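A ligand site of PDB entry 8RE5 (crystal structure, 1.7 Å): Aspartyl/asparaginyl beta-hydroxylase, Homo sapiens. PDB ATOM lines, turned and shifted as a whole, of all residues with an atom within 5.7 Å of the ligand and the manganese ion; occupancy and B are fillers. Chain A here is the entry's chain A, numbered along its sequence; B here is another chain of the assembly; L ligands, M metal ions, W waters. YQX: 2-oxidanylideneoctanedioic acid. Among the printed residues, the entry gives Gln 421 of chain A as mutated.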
ATOM      1  N   LEU A 305       9.249   4.888  29.905  1.00  0.00           N
ATOM      2  CA  LEU A 305       9.198   5.615  28.652  1.00  0.00           C
ATOM      3  C   LEU A 305      10.524   6.276  28.272  1.00  0.00           C
ATOM      4  O   LEU A 305      10.617   6.920  27.215  1.00  0.00           O
ATOM      5  CB  LEU A 305       8.081   6.698  28.695  1.00  0.00           C
ATOM      6  CG  LEU A 305       6.693   6.104  28.929  1.00  0.00           C
ATOM      7  CD1 LEU A 305       5.732   7.313  29.058  1.00  0.00           C
ATOM      8  CD2 LEU A 305       6.284   5.151  27.759  1.00  0.00           C
ATOM      9  N   TRP A 311      13.601  12.603  34.355  1.00  0.00           N
ATOM     10  CA  TRP A 311      12.293  13.195  34.060  1.00  0.00           C
ATOM     11  C   TRP A 311      11.427  12.888  35.263  1.00  0.00           C
ATOM     12  O   TRP A 311      11.270  11.707  35.595  1.00  0.00           O
ATOM     13  CB  TRP A 311      11.725  12.566  32.795  1.00  0.00           C
ATOM     14  CG  TRP A 311      10.331  12.934  32.383  1.00  0.00           C
ATOM     15  CD1 TRP A 311       9.557  14.018  32.779  1.00  0.00           C
ATOM     16  CD2 TRP A 311       9.523  12.176  31.467  1.00  0.00           C
ATOM     17  NE1 TRP A 311       8.289  13.943  32.170  1.00  0.00           N
ATOM     18  CE2 TRP A 311       8.271  12.841  31.340  1.00  0.00           C
ATOM     19  CE3 TRP A 311       9.750  10.995  30.737  1.00  0.00           C
ATOM     20  CZ2 TRP A 311       7.238  12.345  30.483  1.00  0.00           C
ATOM     21  CZ3 TRP A 311       8.744  10.508  29.910  1.00  0.00           C
ATOM     22  CH2 TRP A 311       7.504  11.182  29.766  1.00  0.00           C
ATOM     23  N   SER A 312      10.826  13.898  35.886  1.00  0.00           N
ATOM     24  CA  SER A 312       9.954  13.671  37.055  1.00  0.00           C
ATOM     25  C   SER A 312       8.731  14.560  36.936  1.00  0.00           C
ATOM     26  O   SER A 312       8.751  15.538  36.215  1.00  0.00           O
ATOM     27  CB  SER A 312      10.695  13.982  38.366  1.00  0.00           C
ATOM     28  OG  SER A 312      11.811  13.094  38.497  1.00  0.00           O
ATOM     29  N   GLN A 313       7.646  14.171  37.605  1.00  0.00           N
ATOM     30  CA  GLN A 313       6.368  14.884  37.475  1.00  0.00           C
ATOM     31  C   GLN A 313       5.730  15.061  38.860  1.00  0.00           C
ATOM     32  O   GLN A 313       5.822  14.187  39.726  1.00  0.00           O
ATOM     33  CB  GLN A 313       5.399  14.140  36.497  1.00  0.00           C
ATOM     34  CG  GLN A 313       6.095  13.968  35.118  1.00  0.00           C
ATOM     35  CD  GLN A 313       5.245  13.383  34.000  1.00  0.00           C
ATOM     36  OE1 GLN A 313       5.006  14.085  33.006  1.00  0.00           O
ATOM     37  NE2 GLN A 313       4.862  12.134  34.109  1.00  0.00           N
ATOM     38  N   SER A 354       5.966  19.029  35.045  1.00  0.00           N
ATOM     39  CA  SER A 354       6.925  18.046  34.531  1.00  0.00           C
ATOM     40  C   SER A 354       8.296  18.714  34.435  1.00  0.00           C
ATOM     41  O   SER A 354       8.406  19.794  33.831  1.00  0.00           O
ATOM     42  CB  SER A 354       6.488  17.581  33.162  1.00  0.00           C
ATOM     43  OG  SER A 354       7.452  16.624  32.673  1.00  0.00           O
ATOM     44  N   ILE A 355       9.332  18.090  34.976  1.00  0.00           N
ATOM     45  CA  ILE A 355      10.699  18.603  34.843  1.00  0.00           C
ATOM     46  C   ILE A 355      11.529  17.556  34.101  1.00  0.00           C
ATOM     47  O   ILE A 355      11.452  16.351  34.390  1.00  0.00           O
ATOM     48  CB  ILE A 355      11.307  18.988  36.209  1.00  0.00           C
ATOM     49  CG1 ILE A 355      12.611  19.785  35.992  1.00  0.00           C
ATOM     50  CG2 ILE A 355      11.444  17.734  37.174  1.00  0.00           C
ATOM     51  CD1 ILE A 355      13.217  20.357  37.220  1.00  0.00           C
ATOM     52  N   MET A 356      12.245  18.005  33.068  1.00  0.00           N
ATOM     53  CA  MET A 356      13.097  17.129  32.266  1.00  0.00           C
ATOM     54  C   MET A 356      14.470  17.757  32.125  1.00  0.00           C
ATOM     55  O   MET A 356      14.586  18.945  31.835  1.00  0.00           O
ATOM     56  CB  MET A 356      12.482  16.922  30.895  1.00  0.00           C
ATOM     57  CG  MET A 356      13.151  15.816  30.114  1.00  0.00           C
ATOM     58  SD  MET A 356      12.312  15.460  28.564  1.00  0.00           S
ATOM     59  CE  MET A 356      10.912  14.530  29.116  1.00  0.00           C
ATOM     60  N   VAL A 362      12.981  10.505  25.392  1.00  0.00           N
ATOM     61  CA  VAL A 362      11.788   9.736  25.703  1.00  0.00           C
ATOM     62  C   VAL A 362      11.460   8.955  24.447  1.00  0.00           C
ATOM     63  O   VAL A 362      11.358   9.550  23.364  1.00  0.00           O
ATOM     64  CB  VAL A 362      10.614  10.683  26.072  1.00  0.00           C
ATOM     65  CG1 VAL A 362       9.296   9.934  26.299  1.00  0.00           C
ATOM     66  CG2 VAL A 362      11.034  11.621  27.264  1.00  0.00           C
ATOM     67  N   HIS A 365       6.134   6.970  21.935  1.00  0.00           N
ATOM     68  CA  HIS A 365       5.098   6.287  22.713  1.00  0.00           C
ATOM     69  C   HIS A 365       3.772   6.954  22.431  1.00  0.00           C
ATOM     70  O   HIS A 365       3.681   8.031  21.835  1.00  0.00           O
ATOM     71  CB  HIS A 365       5.384   6.324  24.240  1.00  0.00           C
ATOM     72  CG  HIS A 365       5.353   7.708  24.834  1.00  0.00           C
ATOM     73  ND1 HIS A 365       6.384   8.614  24.659  1.00  0.00           N
ATOM     74  CD2 HIS A 365       4.417   8.350  25.591  1.00  0.00           C
ATOM     75  CE1 HIS A 365       6.080   9.757  25.281  1.00  0.00           C
ATOM     76  NE2 HIS A 365       4.894   9.620  25.853  1.00  0.00           N
ATOM     77  N   GLY A 367      -0.157   7.595  24.515  1.00  0.00           N
ATOM     78  CA  GLY A 367      -0.962   7.488  25.723  1.00  0.00           C
ATOM     79  C   GLY A 367      -2.097   6.482  25.507  1.00  0.00           C
ATOM     80  O   GLY A 367      -2.266   5.943  24.420  1.00  0.00           O
ATOM     81  N   ARG A 374      -3.835  17.009  25.219  1.00  0.00           N
ATOM     82  CA  ARG A 374      -2.795  17.339  26.217  1.00  0.00           C
ATOM     83  C   ARG A 374      -2.275  18.738  25.911  1.00  0.00           C
ATOM     84  O   ARG A 374      -1.710  18.966  24.837  1.00  0.00           O
ATOM     85  CB  ARG A 374      -1.692  16.265  26.223  1.00  0.00           C
ATOM     86  CG  ARG A 374      -0.532  16.595  27.212  1.00  0.00           C
ATOM     87  CD  ARG A 374       0.116  15.269  27.664  1.00  0.00           C
ATOM     88  NE  ARG A 374      -0.739  14.504  28.587  1.00  0.00           N
ATOM     89  CZ  ARG A 374      -0.307  13.480  29.290  1.00  0.00           C
ATOM     90  NH1 ARG A 374       0.900  12.968  29.076  1.00  0.00           N
ATOM     91  NH2 ARG A 374      -1.065  12.986  30.275  1.00  0.00           N
ATOM     92  N   HIS A 376       0.417  21.705  26.955  1.00  0.00           N
ATOM     93  CA  HIS A 376       1.679  22.004  27.616  1.00  0.00           C
ATOM     94  C   HIS A 376       1.802  23.524  27.713  1.00  0.00           C
ATOM     95  O   HIS A 376       1.789  24.204  26.683  1.00  0.00           O
ATOM     96  CB  HIS A 376       2.872  21.516  26.808  1.00  0.00           C
ATOM     97  CG  HIS A 376       3.093  20.044  26.911  1.00  0.00           C
ATOM     98  ND1 HIS A 376       4.196  19.442  26.359  1.00  0.00           N
ATOM     99  CD2 HIS A 376       2.408  19.074  27.558  1.00  0.00           C
ATOM    100  CE1 HIS A 376       4.194  18.159  26.671  1.00  0.00           C
ATOM    101  NE2 HIS A 376       3.103  17.896  27.371  1.00  0.00           N
ATOM    102  N   ILE A 388       9.767  18.419  20.708  1.00  0.00           N
ATOM    103  CA  ILE A 388       8.745  17.377  20.789  1.00  0.00           C
ATOM    104  C   ILE A 388       8.211  17.089  19.390  1.00  0.00           C
ATOM    105  O   ILE A 388       7.781  18.001  18.666  1.00  0.00           O
ATOM    106  CB  ILE A 388       7.581  17.715  21.757  1.00  0.00           C
ATOM    107  CG1 ILE A 388       6.421  16.691  21.667  1.00  0.00           C
ATOM    108  CG2 ILE A 388       7.038  19.144  21.552  1.00  0.00           C
ATOM    109  CD1 ILE A 388       5.460  16.802  22.855  1.00  0.00           C
ATOM    110  N   TRP A 397       8.725  24.379  22.494  1.00  0.00           N
ATOM    111  CA  TRP A 397       7.882  25.135  23.412  1.00  0.00           C
ATOM    112  C   TRP A 397       8.325  26.598  23.517  1.00  0.00           C
ATOM    113  O   TRP A 397       9.435  26.965  23.113  1.00  0.00           O
ATOM    114  CB  TRP A 397       7.972  24.532  24.802  1.00  0.00           C
ATOM    115  CG  TRP A 397       7.524  23.068  24.924  1.00  0.00           C
ATOM    116  CD1 TRP A 397       6.322  22.666  25.383  1.00  0.00           C
ATOM    117  CD2 TRP A 397       8.319  21.901  24.744  1.00  0.00           C
ATOM    118  NE1 TRP A 397       6.268  21.285  25.464  1.00  0.00           N
ATOM    119  CE2 TRP A 397       7.501  20.801  25.093  1.00  0.00           C
ATOM    120  CE3 TRP A 397       9.647  21.659  24.319  1.00  0.00           C
ATOM    121  CZ2 TRP A 397       7.948  19.489  24.993  1.00  0.00           C
ATOM    122  CZ3 TRP A 397      10.065  20.344  24.221  1.00  0.00           C
ATOM    123  CH2 TRP A 397       9.243  19.291  24.594  1.00  0.00           C
ATOM    124  N   PHE A 405      -1.419  19.011  21.872  1.00  0.00           N
ATOM    125  CA  PHE A 405      -1.336  17.854  20.960  1.00  0.00           C
ATOM    126  C   PHE A 405      -2.189  16.718  21.473  1.00  0.00           C
ATOM    127  O   PHE A 405      -2.650  16.675  22.614  1.00  0.00           O
ATOM    128  CB  PHE A 405       0.107  17.346  20.769  1.00  0.00           C
ATOM    129  CG  PHE A 405       0.793  16.876  22.042  1.00  0.00           C
ATOM    130  CD1 PHE A 405       1.226  17.775  22.984  1.00  0.00           C
ATOM    131  CD2 PHE A 405       0.987  15.512  22.284  1.00  0.00           C
ATOM    132  CE1 PHE A 405       1.848  17.376  24.143  1.00  0.00           C
ATOM    133  CE2 PHE A 405       1.652  15.084  23.431  1.00  0.00           C
ATOM    134  CZ  PHE A 405       2.078  16.024  24.386  1.00  0.00           C
ATOM    135  N   ASP A 407      -2.069  13.191  22.484  1.00  0.00           N
ATOM    136  CA  ASP A 407      -0.992  12.265  22.798  1.00  0.00           C
ATOM    137  C   ASP A 407      -1.381  10.809  22.573  1.00  0.00           C
ATOM    138  O   ASP A 407      -0.551   9.920  22.887  1.00  0.00           O
ATOM    139  CB  ASP A 407      -0.458  12.486  24.243  1.00  0.00           C
ATOM    140  CG  ASP A 407      -1.244  11.747  25.333  1.00  0.00           C
ATOM    141  OD1 ASP A 407      -2.495  11.604  25.242  1.00  0.00           O
ATOM    142  OD2 ASP A 407      -0.604  11.402  26.355  1.00  0.00           O
ATOM    143  N   HIS A 411       4.362  10.033  19.925  1.00  0.00           N
ATOM    144  CA  HIS A 411       5.125  11.249  20.103  1.00  0.00           C
ATOM    145  C   HIS A 411       6.416  10.925  20.846  1.00  0.00           C
ATOM    146  O   HIS A 411       6.568   9.841  21.437  1.00  0.00           O
ATOM    147  CB  HIS A 411       4.310  12.313  20.840  1.00  0.00           C
ATOM    148  CG  HIS A 411       3.739  11.847  22.149  1.00  0.00           C
ATOM    149  ND1 HIS A 411       2.698  10.965  22.272  1.00  0.00           N
ATOM    150  CD2 HIS A 411       4.082  12.194  23.419  1.00  0.00           C
ATOM    151  CE1 HIS A 411       2.411  10.783  23.550  1.00  0.00           C
ATOM    152  NE2 HIS A 411       3.248  11.515  24.263  1.00  0.00           N
ATOM    153  N   VAL A 413      10.221  12.895  22.603  1.00  0.00           N
ATOM    154  CA  VAL A 413      10.815  14.132  23.143  1.00  0.00           C
ATOM    155  C   VAL A 413      12.308  13.974  23.342  1.00  0.00           C
ATOM    156  O   VAL A 413      12.803  12.892  23.735  1.00  0.00           O
ATOM    157  CB  VAL A 413      10.117  14.483  24.497  1.00  0.00           C
ATOM    158  CG1 VAL A 413      10.851  15.537  25.234  1.00  0.00           C
ATOM    159  CG2 VAL A 413       8.658  14.885  24.227  1.00  0.00           C
ATOM    160  N   GLN A 421      14.324  21.901  31.978  1.00  0.00           N
ATOM    161  CA  GLN A 421      13.096  22.334  31.315  1.00  0.00           C
ATOM    162  C   GLN A 421      11.911  22.053  32.227  1.00  0.00           C
ATOM    163  O   GLN A 421      11.769  20.927  32.725  1.00  0.00           O
ATOM    164  CB  GLN A 421      12.886  21.555  30.008  1.00  0.00           C
ATOM    165  CG  GLN A 421      11.621  21.984  29.241  1.00  0.00           C
ATOM    166  CD  GLN A 421      11.307  20.952  28.130  1.00  0.00           C
ATOM    167  OE1 GLN A 421      12.026  19.982  27.969  1.00  0.00           O
ATOM    168  NE2 GLN A 421      10.299  21.196  27.352  1.00  0.00           N
ATOM    169  N   LEU A 422      11.055  23.047  32.447  1.00  0.00           N
ATOM    170  CA  LEU A 422       9.892  22.873  33.293  1.00  0.00           C
ATOM    171  C   LEU A 422       8.668  23.210  32.465  1.00  0.00           C
ATOM    172  O   LEU A 422       8.607  24.291  31.867  1.00  0.00           O
ATOM    173  CB  LEU A 422       9.964  23.812  34.516  1.00  0.00           C
ATOM    174  CG  LEU A 422       8.775  23.753  35.522  1.00  0.00           C
ATOM    175  CD1 LEU A 422       8.680  22.379  36.278  1.00  0.00           C
ATOM    176  CD2 LEU A 422       8.901  24.933  36.544  1.00  0.00           C
ATOM    177  N   ILE A 423       7.659  22.319  32.450  1.00  0.00           N
ATOM    178  CA  ILE A 423       6.408  22.622  31.758  1.00  0.00           C
ATOM    179  C   ILE A 423       5.264  22.287  32.696  1.00  0.00           C
ATOM    180  O   ILE A 423       5.442  21.592  33.696  1.00  0.00           O
ATOM    181  CB  ILE A 423       6.245  21.888  30.394  1.00  0.00           C
ATOM    182  CG1 ILE A 423       6.200  20.381  30.569  1.00  0.00           C
ATOM    183  CG2 ILE A 423       7.410  22.300  29.406  1.00  0.00           C
ATOM    184  CD1 ILE A 423       5.727  19.627  29.296  1.00  0.00           C
ATOM    185  N   ILE A 425       1.489  20.539  32.477  1.00  0.00           N
ATOM    186  CA  ILE A 425       0.708  19.676  31.580  1.00  0.00           C
ATOM    187  C   ILE A 425      -0.735  19.710  32.037  1.00  0.00           C
ATOM    188  O   ILE A 425      -1.025  19.441  33.223  1.00  0.00           O
ATOM    189  CB  ILE A 425       1.245  18.245  31.596  1.00  0.00           C
ATOM    190  CG1 ILE A 425       2.731  18.247  31.206  1.00  0.00           C
ATOM    191  CG2 ILE A 425       0.381  17.359  30.684  1.00  0.00           C
ATOM    192  CD1 ILE A 425       3.320  16.865  31.230  1.00  0.00           C
ATOM    193  N   ASP B  18       0.744   8.250  31.218  1.00  0.00           N
ATOM    194  CA  ASP B  18       1.384   8.690  29.987  1.00  0.00           C
ATOM    195  C   ASP B  18       1.458   7.614  28.925  1.00  0.00           C
ATOM    196  O   ASP B  18       1.667   7.944  27.744  1.00  0.00           O
ATOM    197  CB  ASP B  18       2.805   9.145  30.289  1.00  0.00           C
ATOM    198  CG  ASP B  18       2.846  10.393  31.223  1.00  0.00           C
ATOM    199  OD1 ASP B  18       2.035  11.293  30.998  1.00  0.00           O
ATOM    200  OD2 ASP B  18       3.660  10.443  32.175  1.00  0.00           O
HETATM  201  C10 YQX L   1       9.529  18.643  30.641  1.00  0.00           C
HETATM  202  C2  YQX L   1       3.758  14.013  27.243  1.00  0.00           C
HETATM  203  C4  YQX L   1       5.151  13.700  26.714  1.00  0.00           C
HETATM  204  C5  YQX L   1       6.119  14.861  26.682  1.00  0.00           C
HETATM  205  C6  YQX L   1       6.708  15.207  28.049  1.00  0.00           C
HETATM  206  C7  YQX L   1       7.674  16.400  27.958  1.00  0.00           C
HETATM  207  C8  YQX L   1       8.153  16.890  29.351  1.00  0.00           C
HETATM  208  C9  YQX L   1       9.204  18.018  29.296  1.00  0.00           C
HETATM  209  O1  YQX L   1       2.839  13.153  27.026  1.00  0.00           O
HETATM  210  O11 YQX L   1       9.298  17.950  31.656  1.00  0.00           O
HETATM  211  O12 YQX L   1      10.096  19.767  30.684  1.00  0.00           O
HETATM  212  O13 YQX L   1       5.506  12.575  26.326  1.00  0.00           O
HETATM  213  O3  YQX L   1       3.610  15.115  27.903  1.00  0.00           O
HETATM  214 MN    MN M   1       3.691  11.333  26.361  1.00  0.00          MN
HETATM  215  O   HOH W   1       1.875  10.393  26.769  1.00  0.00           O
HETATM  216  O   HOH W   2       3.981  13.524  30.262  1.00  0.00           O
HETATM  217  O   HOH W   3       4.294  11.273  28.505  1.00  0.00           O
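NH1 of Arg 374 is in salt-bridge range of O3 of the ligand (3.7 Å). OG of Ser 354 is in hydrogen-bond range of O11 of the ligand (2.5 Å). N of Met 356 is in hydrogen-bond range of O11 of the ligand, at 3.3 Å. The side-chain amide oxygen of Gln 421 lies close to an oxygen (O12) of the ligand. O of Ser 354 lies close to O11 of the ligand, 3.0 Å away. The backbone carbonyl oxygen of Gln 421 sits close to an oxygen (O12) of the ligand. An oxygen (O11) of the ligand is in hydrogen-bond range of the backbone NH (N) of Ile 355 (3.3 Å). An oxygen (O3) of the ligand sits at hydrogen-bond distance from a ring nitrogen (NE2) of His 376, 2.9 Å away.
The backbone carbonyl oxygen (O) of Val 413 lies within hydrogen-bond range of the backbone NH (N) of Val 362. The side-chain carboxylate (OD2) of Asp 407 is in salt-bridge range of the guanidinium group (NH1) of Arg 374, 3.5 Å away. NH1 of Arg 374 is in salt-bridge range of OD1 of Asp 18 of chain B (2.8 Å). The backbone NH of Ile 355 sits at hydrogen-bond distance from the backbone carbonyl oxygen of Ser 312 (2.9 Å). A ring nitrogen (ND1) of His 376 sits at hydrogen-bond distance from the indole nitrogen of Trp 397. ND1 of His 411 lies close to O of Asp 407 (3.5 Å). N of Gln 421 sits at hydrogen-bond distance from O of Met 356, 3.0 Å away. The side-chain hydroxyl (OG) of Ser 354 sits at hydrogen-bond distance from the indole nitrogen (NE1) of Trp 311, 2.9 Å away.
CZ2 of Trp 311 touches C6 of the ligand (3.8 Å). Phe 405 touches the ligand. Asp 407 touches the ligand. Val 413 touches the ligand (CG2 to C5, 3.5 Å). Leu 422 touches the ligand. Ile 423 touches the ligand (CD1 to C8, 3.7 Å). CD1 of Ile 425 touches O3 of the ligand (3.8 Å). Hydrophobic or aromatic side chains that line the ligand: Trp 311, Met 356, His 365, His 376, Phe 405, His 411, Val 413, Ile 423 and Ile 425. The nearest printed residue that does not touch the ligand is Trp 397 (4.3 Å).
Within 4 Å of the manganese ion: His 365 and His 411.
The manganese ion is bound by water W1 (2.1 Å), O1 of the ligand (2.1 Å), NE2 of His 411 (2.2 Å), NE2 of His 365 (2.2 Å), O13 of the ligand (2.2 Å) and water W3 (2.2 Å).
Water W1 bridges the backbone carbonyl oxygen of Asp 18 of chain B (2.6 Å) and the side-chain carboxylate of Asp 407 (2.7 Å). Water W2 lies within hydrogen-bond range of O3 of the ligand, OE1 of Gln 313, OD1 of Asp 18 of chain B and NH1 of Arg 374.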
